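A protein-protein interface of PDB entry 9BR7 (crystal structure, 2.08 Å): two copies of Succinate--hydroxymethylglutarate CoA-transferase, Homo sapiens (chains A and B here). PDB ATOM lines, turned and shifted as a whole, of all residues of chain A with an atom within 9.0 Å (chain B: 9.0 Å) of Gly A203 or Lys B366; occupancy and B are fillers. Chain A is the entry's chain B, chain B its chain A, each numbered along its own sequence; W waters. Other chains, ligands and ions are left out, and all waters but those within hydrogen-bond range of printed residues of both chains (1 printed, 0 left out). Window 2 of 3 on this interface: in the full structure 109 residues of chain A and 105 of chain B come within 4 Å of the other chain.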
ATOM      1  N   CYS A 100      -2.985   9.131  -0.486  1.00  0.00           N
ATOM      2  CA  CYS A 100      -3.938   9.923   0.270  1.00  0.00           C
ATOM      3  C   CYS A 100      -4.895   9.011   1.023  1.00  0.00           C
ATOM      4  O   CYS A 100      -5.138   7.868   0.625  1.00  0.00           O
ATOM      5  CB  CYS A 100      -4.725  10.868  -0.643  1.00  0.00           C
ATOM      6  SG  CYS A 100      -3.759  12.279  -1.225  1.00  0.00           S
ATOM      7  N   ASP A 101      -5.437   9.534   2.120  1.00  0.00           N
ATOM      8  CA  ASP A 101      -6.331   8.771   2.977  1.00  0.00           C
ATOM      9  C   ASP A 101      -7.798   8.945   2.616  1.00  0.00           C
ATOM     10  O   ASP A 101      -8.594   8.025   2.841  1.00  0.00           O
ATOM     11  CB  ASP A 101      -6.113   9.174   4.436  1.00  0.00           C
ATOM     12  CG  ASP A 101      -4.665   9.047   4.859  1.00  0.00           C
ATOM     13  OD1 ASP A 101      -4.180   7.903   4.973  1.00  0.00           O
ATOM     14  OD2 ASP A 101      -4.010  10.092   5.056  1.00  0.00           O
ATOM     15  N   VAL A 102      -8.175  10.096   2.063  1.00  0.00           N
ATOM     16  CA  VAL A 102      -9.570  10.405   1.783  1.00  0.00           C
ATOM     17  C   VAL A 102      -9.704  10.953   0.369  1.00  0.00           C
ATOM     18  O   VAL A 102      -8.828  11.665  -0.130  1.00  0.00           O
ATOM     19  CB  VAL A 102     -10.143  11.412   2.803  1.00  0.00           C
ATOM     20  CG1 VAL A 102     -11.594  11.731   2.480  1.00  0.00           C
ATOM     21  CG2 VAL A 102     -10.003  10.872   4.221  1.00  0.00           C
ATOM     22  N   TYR A 119     -15.375   5.214  -7.685  1.00  0.00           N
ATOM     23  CA  TYR A 119     -14.940   4.463  -6.513  1.00  0.00           C
ATOM     24  C   TYR A 119     -14.328   3.126  -6.903  1.00  0.00           C
ATOM     25  O   TYR A 119     -13.302   2.720  -6.347  1.00  0.00           O
ATOM     26  CB  TYR A 119     -16.102   4.242  -5.548  1.00  0.00           C
ATOM     27  CG  TYR A 119     -15.696   3.398  -4.362  1.00  0.00           C
ATOM     28  CD1 TYR A 119     -14.841   3.901  -3.393  1.00  0.00           C
ATOM     29  CD2 TYR A 119     -16.141   2.089  -4.228  1.00  0.00           C
ATOM     30  CE1 TYR A 119     -14.453   3.134  -2.312  1.00  0.00           C
ATOM     31  CE2 TYR A 119     -15.757   1.312  -3.149  1.00  0.00           C
ATOM     32  CZ  TYR A 119     -14.914   1.841  -2.195  1.00  0.00           C
ATOM     33  OH  TYR A 119     -14.526   1.076  -1.120  1.00  0.00           O
ATOM     34  N   ASP A 123     -10.607   2.502  -5.683  1.00  0.00           N
ATOM     35  CA  ASP A 123     -10.413   1.463  -4.675  1.00  0.00           C
ATOM     36  C   ASP A 123      -9.475   0.369  -5.167  1.00  0.00           C
ATOM     37  O   ASP A 123      -8.748  -0.231  -4.367  1.00  0.00           O
ATOM     38  CB  ASP A 123     -11.760   0.867  -4.269  1.00  0.00           C
ATOM     39  CG  ASP A 123     -11.620  -0.251  -3.256  1.00  0.00           C
ATOM     40  OD1 ASP A 123     -11.172   0.024  -2.124  1.00  0.00           O
ATOM     41  OD2 ASP A 123     -11.962  -1.404  -3.588  1.00  0.00           O
ATOM     42  N   ALA A 126      -6.146   1.888  -4.575  1.00  0.00           N
ATOM     43  CA  ALA A 126      -6.053   2.491  -3.245  1.00  0.00           C
ATOM     44  C   ALA A 126      -7.100   1.857  -2.341  1.00  0.00           C
ATOM     45  O   ALA A 126      -8.069   2.503  -1.925  1.00  0.00           O
ATOM     46  CB  ALA A 126      -6.227   4.010  -3.319  1.00  0.00           C
ATOM     47  N   PRO A 127      -6.925   0.576  -2.003  1.00  0.00           N
ATOM     48  CA  PRO A 127      -7.932  -0.122  -1.183  1.00  0.00           C
ATOM     49  C   PRO A 127      -8.122   0.473   0.203  1.00  0.00           C
ATOM     50  O   PRO A 127      -9.069   0.083   0.899  1.00  0.00           O
ATOM     51  CB  PRO A 127      -7.387  -1.555  -1.102  1.00  0.00           C
ATOM     52  CG  PRO A 127      -5.915  -1.414  -1.339  1.00  0.00           C
ATOM     53  CD  PRO A 127      -5.761  -0.277  -2.302  1.00  0.00           C
ATOM     54  N   HIS A 128      -7.255   1.390   0.625  1.00  0.00           N
ATOM     55  CA  HIS A 128      -7.350   2.054   1.919  1.00  0.00           C
ATOM     56  C   HIS A 128      -8.243   3.287   1.900  1.00  0.00           C
ATOM     57  O   HIS A 128      -8.570   3.814   2.969  1.00  0.00           O
ATOM     58  CB  HIS A 128      -5.957   2.483   2.377  1.00  0.00           C
ATOM     59  CG  HIS A 128      -5.319   3.483   1.463  1.00  0.00           C
ATOM     60  ND1 HIS A 128      -4.572   3.116   0.365  1.00  0.00           N
ATOM     61  CD2 HIS A 128      -5.350   4.836   1.462  1.00  0.00           C
ATOM     62  CE1 HIS A 128      -4.154   4.200  -0.263  1.00  0.00           C
ATOM     63  NE2 HIS A 128      -4.612   5.258   0.382  1.00  0.00           N
ATOM     64  N   ILE A 129      -8.647   3.752   0.718  1.00  0.00           N
ATOM     65  CA  ILE A 129      -9.161   5.107   0.584  1.00  0.00           C
ATOM     66  C   ILE A 129     -10.561   5.206   1.174  1.00  0.00           C
ATOM     67  O   ILE A 129     -11.376   4.279   1.061  1.00  0.00           O
ATOM     68  CB  ILE A 129      -9.149   5.525  -0.896  1.00  0.00           C
ATOM     69  CG1 ILE A 129      -9.246   7.045  -1.041  1.00  0.00           C
ATOM     70  CG2 ILE A 129     -10.279   4.844  -1.651  1.00  0.00           C
ATOM     71  CD1 ILE A 129      -7.970   7.775  -0.690  1.00  0.00           C
ATOM     72  N   ILE A 130     -10.846   6.340   1.806  1.00  0.00           N
ATOM     73  CA  ILE A 130     -12.193   6.699   2.229  1.00  0.00           C
ATOM     74  C   ILE A 130     -12.761   7.582   1.127  1.00  0.00           C
ATOM     75  O   ILE A 130     -12.323   8.724   0.945  1.00  0.00           O
ATOM     76  CB  ILE A 130     -12.196   7.416   3.586  1.00  0.00           C
ATOM     77  CG1 ILE A 130     -11.498   6.564   4.648  1.00  0.00           C
ATOM     78  CG2 ILE A 130     -13.622   7.728   4.017  1.00  0.00           C
ATOM     79  CD1 ILE A 130     -12.137   5.211   4.869  1.00  0.00           C
ATOM     80  N   TYR A 131     -13.736   7.059   0.392  1.00  0.00           N
ATOM     81  CA  TYR A 131     -14.275   7.714  -0.796  1.00  0.00           C
ATOM     82  C   TYR A 131     -15.649   8.268  -0.445  1.00  0.00           C
ATOM     83  O   TYR A 131     -16.586   7.504  -0.187  1.00  0.00           O
ATOM     84  CB  TYR A 131     -14.349   6.719  -1.953  1.00  0.00           C
ATOM     85  CG  TYR A 131     -14.499   7.323  -3.332  1.00  0.00           C
ATOM     86  CD1 TYR A 131     -15.656   7.995  -3.703  1.00  0.00           C
ATOM     87  CD2 TYR A 131     -13.485   7.198  -4.273  1.00  0.00           C
ATOM     88  CE1 TYR A 131     -15.792   8.536  -4.970  1.00  0.00           C
ATOM     89  CE2 TYR A 131     -13.611   7.734  -5.541  1.00  0.00           C
ATOM     90  CZ  TYR A 131     -14.765   8.403  -5.883  1.00  0.00           C
ATOM     91  OH  TYR A 131     -14.896   8.939  -7.143  1.00  0.00           O
ATOM     92  N   ALA A 192     -15.452   8.991  10.785  1.00  0.00           N
ATOM     93  CA  ALA A 192     -15.913   7.648  11.117  1.00  0.00           C
ATOM     94  C   ALA A 192     -15.234   6.611  10.234  1.00  0.00           C
ATOM     95  O   ALA A 192     -14.867   5.526  10.702  1.00  0.00           O
ATOM     96  CB  ALA A 192     -17.433   7.562  10.981  1.00  0.00           C
ATOM     97  N   GLY A 193     -15.054   6.927   8.950  1.00  0.00           N
ATOM     98  CA  GLY A 193     -14.329   6.023   8.073  1.00  0.00           C
ATOM     99  C   GLY A 193     -12.883   5.841   8.495  1.00  0.00           C
ATOM    100  O   GLY A 193     -12.356   4.727   8.479  1.00  0.00           O
ATOM    101  N   LEU A 194     -12.222   6.938   8.871  1.00  0.00           N
ATOM    102  CA  LEU A 194     -10.847   6.848   9.347  1.00  0.00           C
ATOM    103  C   LEU A 194     -10.744   5.949  10.575  1.00  0.00           C
ATOM    104  O   LEU A 194      -9.866   5.083  10.654  1.00  0.00           O
ATOM    105  CB  LEU A 194     -10.317   8.249   9.656  1.00  0.00           C
ATOM    106  CG  LEU A 194     -10.154   9.184   8.456  1.00  0.00           C
ATOM    107  CD1 LEU A 194      -9.739  10.570   8.923  1.00  0.00           C
ATOM    108  CD2 LEU A 194      -9.151   8.621   7.459  1.00  0.00           C
ATOM    109  N   GLN A 196     -12.788   3.558  11.507  1.00  0.00           N
ATOM    110  CA  GLN A 196     -13.051   2.194  11.066  1.00  0.00           C
ATOM    111  C   GLN A 196     -11.824   1.588  10.386  1.00  0.00           C
ATOM    112  O   GLN A 196     -11.559   0.390  10.535  1.00  0.00           O
ATOM    113  CB  GLN A 196     -14.297   2.203  10.160  1.00  0.00           C
ATOM    114  CG  GLN A 196     -14.845   0.844   9.728  1.00  0.00           C
ATOM    115  CD  GLN A 196     -14.392   0.440   8.340  1.00  0.00           C
ATOM    116  OE1 GLN A 196     -13.821   1.245   7.604  1.00  0.00           O
ATOM    117  NE2 GLN A 196     -14.630  -0.816   7.981  1.00  0.00           N
ATOM    118  N   LYS A 197     -11.068   2.397   9.637  1.00  0.00           N
ATOM    119  CA  LYS A 197      -9.852   1.896   9.000  1.00  0.00           C
ATOM    120  C   LYS A 197      -8.837   1.398  10.028  1.00  0.00           C
ATOM    121  O   LYS A 197      -8.069   0.473   9.737  1.00  0.00           O
ATOM    122  CB  LYS A 197      -9.225   2.974   8.114  1.00  0.00           C
ATOM    123  CG  LYS A 197      -8.019   2.479   7.332  1.00  0.00           C
ATOM    124  CD  LYS A 197      -7.390   3.590   6.515  1.00  0.00           C
ATOM    125  CE  LYS A 197      -6.704   4.608   7.409  1.00  0.00           C
ATOM    126  NZ  LYS A 197      -6.046   5.687   6.620  1.00  0.00           N
ATOM    127  N   TYR A 198      -8.815   1.990  11.229  1.00  0.00           N
ATOM    128  CA  TYR A 198      -7.901   1.519  12.268  1.00  0.00           C
ATOM    129  C   TYR A 198      -8.102   0.042  12.554  1.00  0.00           C
ATOM    130  O   TYR A 198      -7.139  -0.676  12.854  1.00  0.00           O
ATOM    131  CB  TYR A 198      -8.132   2.282  13.577  1.00  0.00           C
ATOM    132  CG  TYR A 198      -7.282   3.501  13.847  1.00  0.00           C
ATOM    133  CD1 TYR A 198      -5.920   3.376  14.080  1.00  0.00           C
ATOM    134  CD2 TYR A 198      -7.847   4.768  13.918  1.00  0.00           C
ATOM    135  CE1 TYR A 198      -5.138   4.479  14.356  1.00  0.00           C
ATOM    136  CE2 TYR A 198      -7.069   5.882  14.190  1.00  0.00           C
ATOM    137  CZ  TYR A 198      -5.715   5.729  14.407  1.00  0.00           C
ATOM    138  OH  TYR A 198      -4.931   6.826  14.678  1.00  0.00           O
ATOM    139  N   THR A 200     -10.002  -2.265  10.370  1.00  0.00           N
ATOM    140  CA  THR A 200     -10.014  -3.107   9.183  1.00  0.00           C
ATOM    141  C   THR A 200      -8.817  -2.897   8.268  1.00  0.00           C
ATOM    142  O   THR A 200      -8.508  -3.791   7.471  1.00  0.00           O
ATOM    143  CB  THR A 200     -11.291  -2.857   8.373  1.00  0.00           C
ATOM    144  OG1 THR A 200     -11.256  -1.531   7.832  1.00  0.00           O
ATOM    145  CG2 THR A 200     -12.516  -2.996   9.261  1.00  0.00           C
ATOM    146  N   GLY A 201      -8.140  -1.752   8.352  1.00  0.00           N
ATOM    147  CA  GLY A 201      -7.080  -1.469   7.410  1.00  0.00           C
ATOM    148  C   GLY A 201      -7.559  -1.182   6.006  1.00  0.00           C
ATOM    149  O   GLY A 201      -6.729  -1.007   5.107  1.00  0.00           O
ATOM    150  N   LYS A 202      -8.869  -1.140   5.789  1.00  0.00           N
ATOM    151  CA  LYS A 202      -9.462  -0.924   4.482  1.00  0.00           C
ATOM    152  C   LYS A 202     -10.329   0.327   4.504  1.00  0.00           C
ATOM    153  O   LYS A 202     -10.772   0.785   5.561  1.00  0.00           O
ATOM    154  CB  LYS A 202     -10.308  -2.132   4.070  1.00  0.00           C
ATOM    155  CG  LYS A 202      -9.500  -3.393   3.843  1.00  0.00           C
ATOM    156  CD  LYS A 202     -10.398  -4.557   3.475  1.00  0.00           C
ATOM    157  CE  LYS A 202      -9.597  -5.839   3.362  1.00  0.00           C
ATOM    158  NZ  LYS A 202      -8.553  -5.735   2.312  1.00  0.00           N
ATOM    159  N   GLY A 203     -10.560   0.882   3.316  1.00  0.00           N
ATOM    160  CA  GLY A 203     -11.411   2.039   3.159  1.00  0.00           C
ATOM    161  C   GLY A 203     -12.854   1.640   2.925  1.00  0.00           C
ATOM    162  O   GLY A 203     -13.256   0.490   3.112  1.00  0.00           O
ATOM    163  N   LEU A 204     -13.646   2.618   2.500  1.00  0.00           N
ATOM    164  CA  LEU A 204     -15.056   2.372   2.231  1.00  0.00           C
ATOM    165  C   LEU A 204     -15.610   3.544   1.433  1.00  0.00           C
ATOM    166  O   LEU A 204     -14.934   4.555   1.227  1.00  0.00           O
ATOM    167  CB  LEU A 204     -15.843   2.156   3.529  1.00  0.00           C
ATOM    168  CG  LEU A 204     -15.852   3.281   4.568  1.00  0.00           C
ATOM    169  CD1 LEU A 204     -16.804   4.393   4.160  1.00  0.00           C
ATOM    170  CD2 LEU A 204     -16.227   2.734   5.939  1.00  0.00           C
ATOM    171  N   PHE A 205     -16.859   3.397   0.999  1.00  0.00           N
ATOM    172  CA  PHE A 205     -17.558   4.419   0.236  1.00  0.00           C
ATOM    173  C   PHE A 205     -18.634   5.057   1.104  1.00  0.00           C
ATOM    174  O   PHE A 205     -19.332   4.364   1.852  1.00  0.00           O
ATOM    175  CB  PHE A 205     -18.182   3.821  -1.029  1.00  0.00           C
ATOM    176  CG  PHE A 205     -18.960   4.811  -1.853  1.00  0.00           C
ATOM    177  CD1 PHE A 205     -18.320   5.609  -2.787  1.00  0.00           C
ATOM    178  CD2 PHE A 205     -20.331   4.937  -1.699  1.00  0.00           C
ATOM    179  CE1 PHE A 205     -19.032   6.518  -3.550  1.00  0.00           C
ATOM    180  CE2 PHE A 205     -21.049   5.845  -2.458  1.00  0.00           C
ATOM    181  CZ  PHE A 205     -20.398   6.637  -3.384  1.00  0.00           C
ATOM    182  N   ILE A 206     -18.760   6.378   1.007  1.00  0.00           N
ATOM    183  CA  ILE A 206     -19.703   7.150   1.808  1.00  0.00           C
ATOM    184  C   ILE A 206     -20.621   7.919   0.867  1.00  0.00           C
ATOM    185  O   ILE A 206     -20.147   8.601  -0.049  1.00  0.00           O
ATOM    186  CB  ILE A 206     -18.983   8.113   2.767  1.00  0.00           C
ATOM    187  CG1 ILE A 206     -18.021   7.346   3.676  1.00  0.00           C
ATOM    188  CG2 ILE A 206     -19.994   8.896   3.596  1.00  0.00           C
ATOM    189  CD1 ILE A 206     -17.204   8.236   4.586  1.00  0.00           C
ATOM    190  N   ASP A 207     -21.927   7.814   1.099  1.00  0.00           N
ATOM    191  CA  ASP A 207     -22.935   8.509   0.303  1.00  0.00           C
ATOM    192  C   ASP A 207     -23.604   9.557   1.187  1.00  0.00           C
ATOM    193  O   ASP A 207     -24.374   9.214   2.091  1.00  0.00           O
ATOM    194  CB  ASP A 207     -23.960   7.530  -0.267  1.00  0.00           C
ATOM    195  CG  ASP A 207     -25.079   8.227  -1.039  1.00  0.00           C
ATOM    196  OD1 ASP A 207     -25.112   9.475  -1.072  1.00  0.00           O
ATOM    197  OD2 ASP A 207     -25.929   7.520  -1.620  1.00  0.00           O
ATOM    198  N   ASN B  11     -21.063  -5.218   8.515  1.00  0.00           N
ATOM    199  CA  ASN B  11     -21.571  -6.019   9.622  1.00  0.00           C
ATOM    200  C   ASN B  11     -21.334  -5.300  10.947  1.00  0.00           C
ATOM    201  O   ASN B  11     -22.257  -5.119  11.742  1.00  0.00           O
ATOM    202  CB  ASN B  11     -20.907  -7.399   9.636  1.00  0.00           C
ATOM    203  CG  ASN B  11     -21.833  -8.488  10.143  1.00  0.00           C
ATOM    204  OD1 ASN B  11     -23.055  -8.375  10.044  1.00  0.00           O
ATOM    205  ND2 ASN B  11     -21.254  -9.553  10.686  1.00  0.00           N
ATOM    206  N   ILE B  12     -20.088  -4.886  11.173  1.00  0.00           N
ATOM    207  CA  ILE B  12     -19.685  -4.211  12.401  1.00  0.00           C
ATOM    208  C   ILE B  12     -19.562  -2.720  12.122  1.00  0.00           C
ATOM    209  O   ILE B  12     -18.927  -2.314  11.140  1.00  0.00           O
ATOM    210  CB  ILE B  12     -18.362  -4.780  12.943  1.00  0.00           C
ATOM    211  CG1 ILE B  12     -17.233  -4.567  11.934  1.00  0.00           C
ATOM    212  CG2 ILE B  12     -18.514  -6.256  13.278  1.00  0.00           C
ATOM    213  CD1 ILE B  12     -15.911  -5.168  12.363  1.00  0.00           C
ATOM    214  N   LYS B  13     -20.161  -1.908  12.987  1.00  0.00           N
ATOM    215  CA  LYS B  13     -20.148  -0.466  12.816  1.00  0.00           C
ATOM    216  C   LYS B  13     -18.840   0.125  13.337  1.00  0.00           C
ATOM    217  O   LYS B  13     -18.148  -0.489  14.153  1.00  0.00           O
ATOM    218  CB  LYS B  13     -21.346   0.152  13.530  1.00  0.00           C
ATOM    219  CG  LYS B  13     -22.683  -0.433  13.079  1.00  0.00           C
ATOM    220  CD  LYS B  13     -23.870   0.272  13.724  1.00  0.00           C
ATOM    221  CE  LYS B  13     -25.189  -0.322  13.240  1.00  0.00           C
ATOM    222  NZ  LYS B  13     -26.371   0.455  13.715  1.00  0.00           N
ATOM    223  N   PRO B  14     -18.472   1.321  12.867  1.00  0.00           N
ATOM    224  CA  PRO B  14     -17.143   1.858  13.207  1.00  0.00           C
ATOM    225  C   PRO B  14     -16.987   2.255  14.665  1.00  0.00           C
ATOM    226  O   PRO B  14     -15.860   2.231  15.174  1.00  0.00           O
ATOM    227  CB  PRO B  14     -17.007   3.070  12.275  1.00  0.00           C
ATOM    228  CG  PRO B  14     -18.399   3.449  11.932  1.00  0.00           C
ATOM    229  CD  PRO B  14     -19.185   2.172  11.901  1.00  0.00           C
ATOM    230  N   ARG B 363     -25.112   6.937   4.298  1.00  0.00           N
ATOM    231  CA  ARG B 363     -25.074   5.505   4.033  1.00  0.00           C
ATOM    232  C   ARG B 363     -23.650   5.085   3.699  1.00  0.00           C
ATOM    233  O   ARG B 363     -22.996   5.706   2.852  1.00  0.00           O
ATOM    234  CB  ARG B 363     -26.020   5.128   2.892  1.00  0.00           C
ATOM    235  CG  ARG B 363     -27.443   4.817   3.333  1.00  0.00           C
ATOM    236  CD  ARG B 363     -28.359   4.795   2.126  1.00  0.00           C
ATOM    237  NE  ARG B 363     -28.320   6.076   1.433  1.00  0.00           N
ATOM    238  CZ  ARG B 363     -28.724   6.273   0.185  1.00  0.00           C
ATOM    239  NH1 ARG B 363     -29.206   5.284  -0.550  1.00  0.00           N
ATOM    240  NH2 ARG B 363     -28.637   7.492  -0.339  1.00  0.00           N
ATOM    241  N   TYR B 364     -23.177   4.031   4.360  1.00  0.00           N
ATOM    242  CA  TYR B 364     -21.839   3.494   4.167  1.00  0.00           C
ATOM    243  C   TYR B 364     -21.910   2.145   3.458  1.00  0.00           C
ATOM    244  O   TYR B 364     -22.884   1.401   3.599  1.00  0.00           O
ATOM    245  CB  TYR B 364     -21.115   3.336   5.508  1.00  0.00           C
ATOM    246  CG  TYR B 364     -21.029   4.609   6.322  1.00  0.00           C
ATOM    247  CD1 TYR B 364     -22.138   5.098   7.002  1.00  0.00           C
ATOM    248  CD2 TYR B 364     -19.834   5.309   6.431  1.00  0.00           C
ATOM    249  CE1 TYR B 364     -22.065   6.256   7.751  1.00  0.00           C
ATOM    250  CE2 TYR B 364     -19.751   6.467   7.182  1.00  0.00           C
ATOM    251  CZ  TYR B 364     -20.870   6.936   7.839  1.00  0.00           C
ATOM    252  OH  TYR B 364     -20.794   8.089   8.587  1.00  0.00           O
ATOM    253  N   SER B 365     -20.863   1.836   2.688  1.00  0.00           N
ATOM    254  CA  SER B 365     -20.863   0.617   1.883  1.00  0.00           C
ATOM    255  C   SER B 365     -20.535  -0.624   2.702  1.00  0.00           C
ATOM    256  O   SER B 365     -20.934  -1.732   2.323  1.00  0.00           O
ATOM    257  CB  SER B 365     -19.868   0.749   0.728  1.00  0.00           C
ATOM    258  OG  SER B 365     -18.538   0.890   1.204  1.00  0.00           O
ATOM    259  N   LYS B 366     -19.819  -0.462   3.818  1.00  0.00           N
ATOM    260  CA  LYS B 366     -19.306  -1.586   4.593  1.00  0.00           C
ATOM    261  C   LYS B 366     -20.187  -1.981   5.771  1.00  0.00           C
ATOM    262  O   LYS B 366     -19.902  -2.999   6.411  1.00  0.00           O
ATOM    263  CB  LYS B 366     -17.887  -1.287   5.110  1.00  0.00           C
ATOM    264  CG  LYS B 366     -16.794  -1.284   4.045  1.00  0.00           C
ATOM    265  CD  LYS B 366     -16.519  -2.704   3.540  1.00  0.00           C
ATOM    266  CE  LYS B 366     -15.213  -2.762   2.766  1.00  0.00           C
ATOM    267  NZ  LYS B 366     -14.935  -4.125   2.237  1.00  0.00           N
ATOM    268  N   PHE B 367     -21.235  -1.222   6.074  1.00  0.00           N
ATOM    269  CA  PHE B 367     -22.134  -1.604   7.154  1.00  0.00           C
ATOM    270  C   PHE B 367     -23.481  -0.934   6.940  1.00  0.00           C
ATOM    271  O   PHE B 367     -23.598   0.056   6.212  1.00  0.00           O
ATOM    272  CB  PHE B 367     -21.550  -1.246   8.526  1.00  0.00           C
ATOM    273  CG  PHE B 367     -21.193   0.205   8.680  1.00  0.00           C
ATOM    274  CD1 PHE B 367     -19.945   0.669   8.299  1.00  0.00           C
ATOM    275  CD2 PHE B 367     -22.101   1.102   9.217  1.00  0.00           C
ATOM    276  CE1 PHE B 367     -19.611   2.004   8.445  1.00  0.00           C
ATOM    277  CE2 PHE B 367     -21.774   2.437   9.364  1.00  0.00           C
ATOM    278  CZ  PHE B 367     -20.527   2.888   8.980  1.00  0.00           C
ATOM    279  N   LYS B 368     -24.498  -1.492   7.590  1.00  0.00           N
ATOM    280  CA  LYS B 368     -25.869  -1.018   7.485  1.00  0.00           C
ATOM    281  C   LYS B 368     -26.318  -0.461   8.829  1.00  0.00           C
ATOM    282  O   LYS B 368     -25.962  -0.996   9.884  1.00  0.00           O
ATOM    283  CB  LYS B 368     -26.812  -2.142   7.043  1.00  0.00           C
ATOM    284  CG  LYS B 368     -26.606  -2.609   5.607  1.00  0.00           C
ATOM    285  CD  LYS B 368     -27.612  -3.688   5.227  1.00  0.00           C
ATOM    286  CE  LYS B 368     -27.470  -4.101   3.768  1.00  0.00           C
ATOM    287  NZ  LYS B 368     -28.550  -5.040   3.347  1.00  0.00           N
ATOM    288  N   MET B 369     -27.101   0.616   8.783  1.00  0.00           N
ATOM    289  CA  MET B 369     -27.666   1.225   9.981  1.00  0.00           C
ATOM    290  C   MET B 369     -29.190   1.186   9.966  1.00  0.00           C
ATOM    291  O   MET B 369     -29.836   1.909  10.732  1.00  0.00           O
ATOM    292  CB  MET B 369     -27.165   2.663  10.141  1.00  0.00           C
ATOM    293  CG  MET B 369     -25.647   2.793  10.135  1.00  0.00           C
ATOM    294  SD  MET B 369     -25.070   4.458  10.520  1.00  0.00           S
ATOM    295  CE  MET B 369     -25.673   5.366   9.097  1.00  0.00           C
HETATM  296  O   HOH W   1     -27.347   8.950   1.964  1.00  0.00           O
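The guanidinium group of Arg B363 is in salt-bridge range of the side-chain carboxylate of Asp A207 (3.0 Å). N of Phe A205 lies within hydrogen-bond range of OG of Ser B365.
No position is printed for both chains.
Of the 25 printed residues of chain A, 7 touch a printed residue of chain B. Hydrophobic or aromatic side chains of chain A within 4 Å of the printed part of chain B: Leu A204, Phe A205 and Ile A206. Along chain A the printed residues that touch a printed residue of chain B span positions 192 to 207. Of the 11 printed residues of chain B, 5 touch a printed residue of chain A. Printed residues of chain B that touch a printed residue of chain A: Pro B14, Arg B363, Tyr B364, Ser B365 and Lys B366. Hydrophobic or aromatic side chains of chain B that line the printed part of chain A: Pro B14 and Tyr B364. Among the printed residues, 11 pairs touch across the chains.
Gly A193 touches none of the printed residues of chain B. Printed residues of chain B within 4 Å of Gln A196: Pro B14. Of chain B, only Lys B366 comes within 4 Å of Gly A203. Asn B11 touches none of the printed residues of chain A. Printed residues of chain A within 4 Å of Pro B14: Ala A192 and Gln A196. Lys B366 touches two residues of chain A. The nearest residue of chain B that does not touch Gly A203 is Ser B365 (5.6 Å).
Water W1 bridges the backbone carbonyl oxygen (O) of Asp A207 (3.0 Å) and the guanidinium group (NH2) of Arg B363 (3.0 Å).
O of Ala A192 touches CB of Pro B14, 3.6 Å away. Gln A196 touches Pro B14. Gly A203 touches Lys B366 (O to CE, 3.8 Å). Tyr B364 touches Leu A204. Leu A204 touches Ser B365. Leu A204 touches Lys B366 (CB to CG, 3.6 Å). CA of Tyr B364 touches O of Phe A205, 3.5 Å away. O of Arg B363 touches CA of Ile A206, 3.7 Å away. CD2 of Tyr B364 touches CG1 of Ile A206, 3.9 Å away.
N of Ile A206 lies within hydrogen-bond range of O of Tyr A131 (2.7 Å). The backbone carbonyl oxygen of Pro A127 is in hydrogen-bond range of the backbone NH of Gly A203, at 3.0 Å. O of Ile A129 sits at hydrogen-bond distance from N of Leu A204 (3.2 Å). The backbone carbonyl oxygen of Leu A204 is in hydrogen-bond range of the backbone NH of Tyr A131, 2.9 Å away. The backbone carbonyl oxygen (O) of Lys B366 lies within hydrogen-bond range of the backbone NH (N) of Asn B11. The backbone carbonyl oxygen (O) of Gln A196 is in hydrogen-bond range of the side-chain hydroxyl (OG1) of Thr A200, 3.3 Å away.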
